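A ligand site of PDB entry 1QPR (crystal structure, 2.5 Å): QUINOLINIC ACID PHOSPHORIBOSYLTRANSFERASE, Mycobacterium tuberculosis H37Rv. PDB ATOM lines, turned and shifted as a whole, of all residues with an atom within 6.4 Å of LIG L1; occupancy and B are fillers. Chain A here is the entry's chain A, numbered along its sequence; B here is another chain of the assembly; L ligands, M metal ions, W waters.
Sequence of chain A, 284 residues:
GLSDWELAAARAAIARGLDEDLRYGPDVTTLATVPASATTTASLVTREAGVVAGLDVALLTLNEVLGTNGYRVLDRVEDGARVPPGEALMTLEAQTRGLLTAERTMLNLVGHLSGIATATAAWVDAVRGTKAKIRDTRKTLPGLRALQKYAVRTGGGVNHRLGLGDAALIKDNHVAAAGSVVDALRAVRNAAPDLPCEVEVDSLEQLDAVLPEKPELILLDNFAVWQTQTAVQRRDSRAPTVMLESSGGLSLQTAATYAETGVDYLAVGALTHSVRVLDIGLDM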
ATOM      1  N   ASP A 136      -4.422  -5.733  12.511  1.00  0.00           N
ATOM      2  CA  ASP A 136      -3.198  -6.256  11.977  1.00  0.00           C
ATOM      3  C   ASP A 136      -2.803  -5.530  10.672  1.00  0.00           C
ATOM      4  O   ASP A 136      -3.407  -4.529  10.308  1.00  0.00           O
ATOM      5  CB  ASP A 136      -3.317  -7.761  11.748  1.00  0.00           C
ATOM      6  CG  ASP A 136      -4.653  -8.140  11.102  1.00  0.00           C
ATOM      7  OD1 ASP A 136      -5.103  -7.499  10.123  1.00  0.00           O
ATOM      8  OD2 ASP A 136      -5.260  -9.107  11.571  1.00  0.00           O
ATOM      9  N   THR A 137      -1.808  -6.078   9.988  1.00  0.00           N
ATOM     10  CA  THR A 137      -1.291  -5.535   8.751  1.00  0.00           C
ATOM     11  C   THR A 137      -1.060  -6.630   7.687  1.00  0.00           C
ATOM     12  O   THR A 137      -1.550  -7.758   7.808  1.00  0.00           O
ATOM     13  CB  THR A 137       0.069  -4.858   9.018  1.00  0.00           C
ATOM     14  OG1 THR A 137       1.055  -5.868   9.290  1.00  0.00           O
ATOM     15  CG2 THR A 137      -0.027  -3.858  10.199  1.00  0.00           C
ATOM     16  N   ARG A 138      -0.326  -6.288   6.628  1.00  0.00           N
ATOM     17  CA  ARG A 138       0.008  -7.228   5.587  1.00  0.00           C
ATOM     18  C   ARG A 138       1.420  -7.712   5.828  1.00  0.00           C
ATOM     19  O   ARG A 138       2.022  -8.351   4.996  1.00  0.00           O
ATOM     20  CB  ARG A 138      -0.115  -6.615   4.203  1.00  0.00           C
ATOM     21  CG  ARG A 138      -1.558  -6.541   3.656  1.00  0.00           C
ATOM     22  CD  ARG A 138      -1.522  -6.286   2.153  1.00  0.00           C
ATOM     23  NE  ARG A 138      -0.789  -5.055   1.867  1.00  0.00           N
ATOM     24  CZ  ARG A 138       0.221  -4.947   1.007  1.00  0.00           C
ATOM     25  NH1 ARG A 138       0.632  -5.967   0.296  1.00  0.00           N
ATOM     26  NH2 ARG A 138       0.898  -3.843   0.960  1.00  0.00           N
ATOM     27  N   LYS A 139       1.956  -7.397   7.002  1.00  0.00           N
ATOM     28  CA  LYS A 139       3.271  -7.837   7.320  1.00  0.00           C
ATOM     29  C   LYS A 139       3.115  -9.219   7.912  1.00  0.00           C
ATOM     30  O   LYS A 139       3.368  -9.419   9.096  1.00  0.00           O
ATOM     31  CB  LYS A 139       3.909  -6.874   8.296  1.00  0.00           C
ATOM     32  CG  LYS A 139       3.960  -5.450   7.818  1.00  0.00           C
ATOM     33  CD  LYS A 139       4.597  -4.604   8.867  1.00  0.00           C
ATOM     34  CE  LYS A 139       4.897  -3.225   8.374  1.00  0.00           C
ATOM     35  NZ  LYS A 139       6.375  -2.887   8.522  1.00  0.00           N
ATOM     36  N   LYS A 149      -4.007 -14.174  10.361  1.00  0.00           N
ATOM     37  CA  LYS A 149      -5.129 -13.245  10.422  1.00  0.00           C
ATOM     38  C   LYS A 149      -6.215 -13.845  11.322  1.00  0.00           C
ATOM     39  O   LYS A 149      -6.894 -13.128  12.079  1.00  0.00           O
ATOM     40  CB  LYS A 149      -5.660 -13.028   9.008  1.00  0.00           C
ATOM     41  CG  LYS A 149      -5.812 -11.571   8.582  1.00  0.00           C
ATOM     42  CD  LYS A 149      -4.536 -10.909   8.176  1.00  0.00           C
ATOM     43  CE  LYS A 149      -4.905  -9.495   7.806  1.00  0.00           C
ATOM     44  NZ  LYS A 149      -3.812  -8.559   7.580  1.00  0.00           N
ATOM     45  N   HIS A 160      -7.489  -6.169   9.298  1.00  0.00           N
ATOM     46  CA  HIS A 160      -7.419  -5.046   8.407  1.00  0.00           C
ATOM     47  C   HIS A 160      -7.650  -5.733   7.046  1.00  0.00           C
ATOM     48  O   HIS A 160      -8.212  -6.836   6.973  1.00  0.00           O
ATOM     49  CB  HIS A 160      -6.025  -4.447   8.463  1.00  0.00           C
ATOM     50  CG  HIS A 160      -5.968  -3.052   7.946  1.00  0.00           C
ATOM     51  ND1 HIS A 160      -5.315  -2.039   8.617  1.00  0.00           N
ATOM     52  CD2 HIS A 160      -6.518  -2.478   6.855  1.00  0.00           C
ATOM     53  CE1 HIS A 160      -5.475  -0.906   7.961  1.00  0.00           C
ATOM     54  NE2 HIS A 160      -6.194  -1.146   6.887  1.00  0.00           N
ATOM     55  N   ARG A 161      -7.138  -5.161   5.964  1.00  0.00           N
ATOM     56  CA  ARG A 161      -7.376  -5.781   4.660  1.00  0.00           C
ATOM     57  C   ARG A 161      -6.561  -7.042   4.517  1.00  0.00           C
ATOM     58  O   ARG A 161      -5.541  -7.203   5.172  1.00  0.00           O
ATOM     59  CB  ARG A 161      -7.098  -4.798   3.515  1.00  0.00           C
ATOM     60  CG  ARG A 161      -5.682  -4.332   3.397  1.00  0.00           C
ATOM     61  CD  ARG A 161      -5.591  -3.291   2.287  1.00  0.00           C
ATOM     62  NE  ARG A 161      -4.212  -2.823   2.126  1.00  0.00           N
ATOM     63  CZ  ARG A 161      -3.721  -2.339   0.999  1.00  0.00           C
ATOM     64  NH1 ARG A 161      -4.541  -2.249  -0.026  1.00  0.00           N
ATOM     65  NH2 ARG A 161      -2.415  -2.054   0.870  1.00  0.00           N
ATOM     66  N   LEU A 162      -7.072  -7.973   3.730  1.00  0.00           N
ATOM     67  CA  LEU A 162      -6.443  -9.256   3.492  1.00  0.00           C
ATOM     68  C   LEU A 162      -5.490  -9.247   2.329  1.00  0.00           C
ATOM     69  O   LEU A 162      -4.585 -10.067   2.244  1.00  0.00           O
ATOM     70  CB  LEU A 162      -7.521 -10.336   3.298  1.00  0.00           C
ATOM     71  CG  LEU A 162      -8.562 -10.498   4.421  1.00  0.00           C
ATOM     72  CD1 LEU A 162      -9.600 -11.488   3.977  1.00  0.00           C
ATOM     73  CD2 LEU A 162      -7.960 -10.979   5.722  1.00  0.00           C
ATOM     74  N   GLY A 163      -5.663  -8.281   1.439  1.00  0.00           N
ATOM     75  CA  GLY A 163      -4.808  -8.214   0.291  1.00  0.00           C
ATOM     76  C   GLY A 163      -4.750  -6.821  -0.251  1.00  0.00           C
ATOM     77  O   GLY A 163      -5.128  -5.868   0.418  1.00  0.00           O
ATOM     78  N   LEU A 164      -4.320  -6.734  -1.506  1.00  0.00           N
ATOM     79  CA  LEU A 164      -4.154  -5.468  -2.226  1.00  0.00           C
ATOM     80  C   LEU A 164      -5.423  -4.911  -2.922  1.00  0.00           C
ATOM     81  O   LEU A 164      -5.600  -3.680  -3.040  1.00  0.00           O
ATOM     82  CB  LEU A 164      -3.019  -5.639  -3.247  1.00  0.00           C
ATOM     83  CG  LEU A 164      -1.699  -4.899  -3.123  1.00  0.00           C
ATOM     84  CD1 LEU A 164      -1.478  -4.267  -1.784  1.00  0.00           C
ATOM     85  CD2 LEU A 164      -0.592  -5.828  -3.480  1.00  0.00           C
ATOM     86  N   LEU A 169      -5.314   1.642  -0.029  1.00  0.00           N
ATOM     87  CA  LEU A 169      -4.560   2.220   1.029  1.00  0.00           C
ATOM     88  C   LEU A 169      -3.445   3.002   0.376  1.00  0.00           C
ATOM     89  O   LEU A 169      -2.508   2.410  -0.169  1.00  0.00           O
ATOM     90  CB  LEU A 169      -4.015   1.118   1.934  1.00  0.00           C
ATOM     91  CG  LEU A 169      -3.875   1.435   3.420  1.00  0.00           C
ATOM     92  CD1 LEU A 169      -3.304   0.266   4.147  1.00  0.00           C
ATOM     93  CD2 LEU A 169      -2.992   2.653   3.643  1.00  0.00           C
ATOM     94  N   LYS A 171      -0.166   4.792   0.199  1.00  0.00           N
ATOM     95  CA  LYS A 171       1.069   4.792   0.946  1.00  0.00           C
ATOM     96  C   LYS A 171       2.077   5.840   0.478  1.00  0.00           C
ATOM     97  O   LYS A 171       1.898   6.441  -0.568  1.00  0.00           O
ATOM     98  CB  LYS A 171       1.670   3.391   0.882  1.00  0.00           C
ATOM     99  CG  LYS A 171       0.836   2.348   1.581  1.00  0.00           C
ATOM    100  CD  LYS A 171       1.355   0.928   1.329  1.00  0.00           C
ATOM    101  CE  LYS A 171       0.815  -0.108   2.355  1.00  0.00           C
ATOM    102  NZ  LYS A 171       1.319   0.166   3.706  1.00  0.00           N
ATOM    103  N   GLU A 198      -8.263   4.332   2.325  1.00  0.00           N
ATOM    104  CA  GLU A 198      -7.480   4.708   3.464  1.00  0.00           C
ATOM    105  C   GLU A 198      -6.256   5.395   2.914  1.00  0.00           C
ATOM    106  O   GLU A 198      -5.612   4.910   2.000  1.00  0.00           O
ATOM    107  CB  GLU A 198      -7.044   3.447   4.217  1.00  0.00           C
ATOM    108  CG  GLU A 198      -8.223   2.519   4.581  1.00  0.00           C
ATOM    109  CD  GLU A 198      -8.016   1.020   4.251  1.00  0.00           C
ATOM    110  OE1 GLU A 198      -6.904   0.641   3.824  1.00  0.00           O
ATOM    111  OE2 GLU A 198      -8.988   0.217   4.438  1.00  0.00           O
ATOM    112  N   GLU A 200      -2.524   7.235   3.932  1.00  0.00           N
ATOM    113  CA  GLU A 200      -1.480   7.319   4.924  1.00  0.00           C
ATOM    114  C   GLU A 200      -0.800   8.710   4.927  1.00  0.00           C
ATOM    115  O   GLU A 200      -0.312   9.186   3.878  1.00  0.00           O
ATOM    116  CB  GLU A 200      -0.497   6.202   4.581  1.00  0.00           C
ATOM    117  CG  GLU A 200       0.771   6.134   5.343  1.00  0.00           C
ATOM    118  CD  GLU A 200       1.635   4.975   4.860  1.00  0.00           C
ATOM    119  OE1 GLU A 200       1.167   3.807   4.932  1.00  0.00           O
ATOM    120  OE2 GLU A 200       2.766   5.247   4.382  1.00  0.00           O
ATOM    121  N   LEU A 219      -4.421   6.866   8.093  1.00  0.00           N
ATOM    122  CA  LEU A 219      -3.416   6.165   8.850  1.00  0.00           C
ATOM    123  C   LEU A 219      -2.356   7.172   9.294  1.00  0.00           C
ATOM    124  O   LEU A 219      -1.609   7.703   8.469  1.00  0.00           O
ATOM    125  CB  LEU A 219      -2.796   5.048   7.998  1.00  0.00           C
ATOM    126  CG  LEU A 219      -1.841   4.065   8.664  1.00  0.00           C
ATOM    127  CD1 LEU A 219      -2.045   2.719   8.075  1.00  0.00           C
ATOM    128  CD2 LEU A 219      -0.409   4.499   8.479  1.00  0.00           C
ATOM    129  N   GLU A 245      -6.404   5.805  12.276  1.00  0.00           N
ATOM    130  CA  GLU A 245      -5.690   4.581  12.625  1.00  0.00           C
ATOM    131  C   GLU A 245      -4.225   4.853  12.863  1.00  0.00           C
ATOM    132  O   GLU A 245      -3.552   5.341  11.963  1.00  0.00           O
ATOM    133  CB  GLU A 245      -5.825   3.591  11.483  1.00  0.00           C
ATOM    134  CG  GLU A 245      -4.971   2.360  11.607  1.00  0.00           C
ATOM    135  CD  GLU A 245      -5.505   1.215  10.764  1.00  0.00           C
ATOM    136  OE1 GLU A 245      -5.750   1.428   9.571  1.00  0.00           O
ATOM    137  OE2 GLU A 245      -5.716   0.104  11.281  1.00  0.00           O
ATOM    138  N   SER A 247      -0.343   3.887  13.287  1.00  0.00           N
ATOM    139  CA  SER A 247       0.539   2.822  12.864  1.00  0.00           C
ATOM    140  C   SER A 247       1.961   3.361  12.778  1.00  0.00           C
ATOM    141  O   SER A 247       2.159   4.524  12.416  1.00  0.00           O
ATOM    142  CB  SER A 247       0.083   2.264  11.514  1.00  0.00           C
ATOM    143  OG  SER A 247       0.722   1.025  11.270  1.00  0.00           O
ATOM    144  N   ALA A 267      -2.871  -0.123  14.460  1.00  0.00           N
ATOM    145  CA  ALA A 267      -2.468  -1.129  13.469  1.00  0.00           C
ATOM    146  C   ALA A 267      -1.076  -1.623  13.886  1.00  0.00           C
ATOM    147  O   ALA A 267      -0.082  -0.850  13.792  1.00  0.00           O
ATOM    148  CB  ALA A 267      -2.416  -0.512  12.094  1.00  0.00           C
ATOM    149  N   VAL A 268      -0.999  -2.878  14.339  1.00  0.00           N
ATOM    150  CA  VAL A 268       0.238  -3.450  14.867  1.00  0.00           C
ATOM    151  C   VAL A 268       0.904  -4.509  14.013  1.00  0.00           C
ATOM    152  O   VAL A 268       0.470  -5.652  13.947  1.00  0.00           O
ATOM    153  CB  VAL A 268      -0.009  -4.011  16.313  1.00  0.00           C
ATOM    154  CG1 VAL A 268       1.338  -4.240  17.053  1.00  0.00           C
ATOM    155  CG2 VAL A 268      -0.891  -3.052  17.148  1.00  0.00           C
ATOM    156  N   GLY A 269       2.041  -4.153  13.457  1.00  0.00           N
ATOM    157  CA  GLY A 269       2.761  -5.097  12.615  1.00  0.00           C
ATOM    158  C   GLY A 269       3.391  -6.238  13.379  1.00  0.00           C
ATOM    159  O   GLY A 269       3.431  -7.368  12.921  1.00  0.00           O
ATOM    160  N   ARG B 104       5.600  -5.490  -0.540  1.00  0.00           N
ATOM    161  CA  ARG B 104       5.311  -6.193   0.704  1.00  0.00           C
ATOM    162  C   ARG B 104       5.798  -7.642   0.797  1.00  0.00           C
ATOM    163  O   ARG B 104       6.385  -8.010   1.785  1.00  0.00           O
ATOM    164  CB  ARG B 104       3.834  -6.081   1.054  1.00  0.00           C
ATOM    165  CG  ARG B 104       3.455  -6.736   2.363  1.00  0.00           C
ATOM    166  CD  ARG B 104       4.282  -6.256   3.546  1.00  0.00           C
ATOM    167  NE  ARG B 104       4.167  -4.817   3.758  1.00  0.00           N
ATOM    168  CZ  ARG B 104       5.160  -4.058   4.203  1.00  0.00           C
ATOM    169  NH1 ARG B 104       6.353  -4.594   4.496  1.00  0.00           N
ATOM    170  NH2 ARG B 104       4.958  -2.750   4.349  1.00  0.00           N
ATOM    171  N   ASN B 108       8.620  -8.671   3.356  1.00  0.00           N
ATOM    172  CA  ASN B 108       8.279  -9.664   4.391  1.00  0.00           C
ATOM    173  C   ASN B 108       9.274 -10.858   4.459  1.00  0.00           C
ATOM    174  O   ASN B 108       9.596 -11.344   5.555  1.00  0.00           O
ATOM    175  CB  ASN B 108       6.858 -10.179   4.163  1.00  0.00           C
ATOM    176  CG  ASN B 108       5.804  -9.167   4.506  1.00  0.00           C
ATOM    177  OD1 ASN B 108       6.074  -8.188   5.214  1.00  0.00           O
ATOM    178  ND2 ASN B 108       4.601  -9.383   4.017  1.00  0.00           N
HETATM  179  O1  LIG L   1      -1.034  -2.772   3.535  1.00  0.00           O
HETATM  180  O2  LIG L   1      -2.756  -3.580   4.654  1.00  0.00           O
HETATM  181  C1  LIG L   1       1.332  -2.806   5.583  1.00  0.00           C
HETATM  182  O3  LIG L   1       2.204  -2.023   5.109  1.00  0.00           O
HETATM  183  O4  LIG L   1       1.454  -4.045   5.415  1.00  0.00           O
HETATM  184  C2  LIG L   1      -1.674  -2.957   4.646  1.00  0.00           C
HETATM  185  C3  LIG L   1       0.466  -1.739   7.609  1.00  0.00           C
HETATM  186  C4  LIG L   1       0.180  -2.308   6.369  1.00  0.00           C
HETATM  187  C5  LIG L   1      -1.142  -2.394   5.971  1.00  0.00           C
HETATM  188  C6  LIG L   1      -2.123  -1.900   6.868  1.00  0.00           C
HETATM  189  C7  LIG L   1      -1.777  -1.257   8.030  1.00  0.00           C
HETATM  190  C8  LIG L   1      -0.469  -1.222   8.398  1.00  0.00           C
HETATM  191  C1  LG2 L   2       3.965   0.045   7.305  1.00  0.00           C
HETATM  192  C2  LG2 L   2       2.846   0.758   7.832  1.00  0.00           C
HETATM  193  C3  LG2 L   2       3.181   1.171   9.110  1.00  0.00           C
HETATM  194  C4  LG2 L   2       3.949   0.198   9.708  1.00  0.00           C
HETATM  195  C5  LG2 L   2       3.143  -1.147  10.186  1.00  0.00           C
HETATM  196  O1  LG2 L   2       4.948   0.851   6.410  1.00  0.00           O
HETATM  197  O2  LG2 L   2       2.142   1.813   6.741  1.00  0.00           O
HETATM  198  O3  LG2 L   2       4.143   2.391   9.121  1.00  0.00           O
HETATM  199  P1  LG2 L   2       4.740  -1.853  12.342  1.00  0.00           P
HETATM  200  O4  LG2 L   2       5.581  -0.707  12.326  1.00  0.00           O
HETATM  201  O5  LG2 L   2       4.502  -2.297  13.654  1.00  0.00           O
HETATM  202  O6  LG2 L   2       5.412  -2.829  11.606  1.00  0.00           O
HETATM  203  P2  LG2 L   2       6.679   0.371   6.390  1.00  0.00           P
HETATM  204  O7  LG2 L   2       7.132   0.175   7.933  1.00  0.00           O
HETATM  205  O8  LG2 L   2       6.885  -0.996   5.613  1.00  0.00           O
HETATM  206  P3  LG2 L   2       7.759   3.053   6.460  1.00  0.00           P
HETATM  207  O9  LG2 L   2       6.168   3.753   6.903  1.00  0.00           O
HETATM  208  O10 LG2 L   2       8.570   4.176   5.460  1.00  0.00           O
HETATM  209  O11 LG2 L   2       8.658   2.903   7.903  1.00  0.00           O
HETATM  210  C6  LG2 L   2       7.657   1.554   5.625  1.00  0.00           C
HETATM  211  O12 LG2 L   2       3.242  -1.452  11.745  1.00  0.00           O
HETATM  212  O13 LG2 L   2       4.727  -0.261   8.492  1.00  0.00           O
HETATM  213 MN    MN M   1       4.118   2.779   6.810  1.00  0.00          MN
HETATM  214  O   HOH W   1      -3.635  -5.562   6.401  1.00  0.00           O
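The side-chain amino group (NZ) of Lys 171 lies within salt-bridge range of an oxygen (O3) of LIG L1, at 2.7 Å. The backbone NH of Arg 138 is in hydrogen-bond range of an oxygen (O4) of LIG L1, at 3.1 Å. The guanidinium group of Arg 138 is in salt-bridge range of an oxygen (O1) of LIG L1 (2.8 Å). O3 of LIG L1 is in salt-bridge range of NH2 of Arg 104 of chain B (2.9 Å). An oxygen (O2) of LIG L1 is in salt-bridge range of the guanidinium group (NE) of Arg 161, 3.0 Å away. The guanidinium group (NH2) of Arg 104 of chain B lies within salt-bridge range of an oxygen (O8) of LG2 L2. An oxygen (O6) of LG2 L2 is in salt-bridge range of the side-chain amino group (NZ) of Lys 139 (3.2 Å). An oxygen (O2) of LG2 L2 sits close to the side-chain carboxylate of Glu 200. The backbone NH (N) of Gly 269 lies within hydrogen-bond range of an oxygen (O5) of LG2 L2 (3.1 Å).
NZ of Lys 171 lies within salt-bridge range of OE1 of Glu 200 (3.8 Å). ND2 of Asn 108 of chain B lies within hydrogen-bond range of O of Arg 138 (2.9 Å). O of Arg 104 of chain B lies close to ND2 of Asn 108 of chain B (3.2 Å). O of Arg 161 sits at hydrogen-bond distance from NZ of Lys 149, 3.3 Å away. N of Lys 139 is in hydrogen-bond range of OG1 of Thr 137. The backbone NH (N) of His 160 is in hydrogen-bond range of the side-chain carboxylate (OD1) of Asp 136 (2.9 Å). A ring nitrogen (ND1) of His 160 lies within hydrogen-bond range of the side-chain carboxylate (OE2) of Glu 245, 3.4 Å away. OG of Ser 247 is in hydrogen-bond range of O of Ala 267.
Merely in contact with LIG L1: Thr 137, His 160, Leu 169, Lys 139, Ser 247 and Leu 219. Of the 22 residues printed, 10 come within 4 Å of LIG L1. The nearest printed residue that does not touch LIG L1 is Ala 267 (4.2 Å).
Water W1 lies within hydrogen-bond range of an oxygen (O2) of LIG L1 (2.8 Å), the backbone carbonyl oxygen (O) of Arg 161 (2.8 Å), the side-chain amino group (NZ) of Lys 149 (3.2 Å), the backbone carbonyl oxygen (O) of Thr 137 (3.3 Å) and the backbone NH (N) of Arg 138 (3.4 Å).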
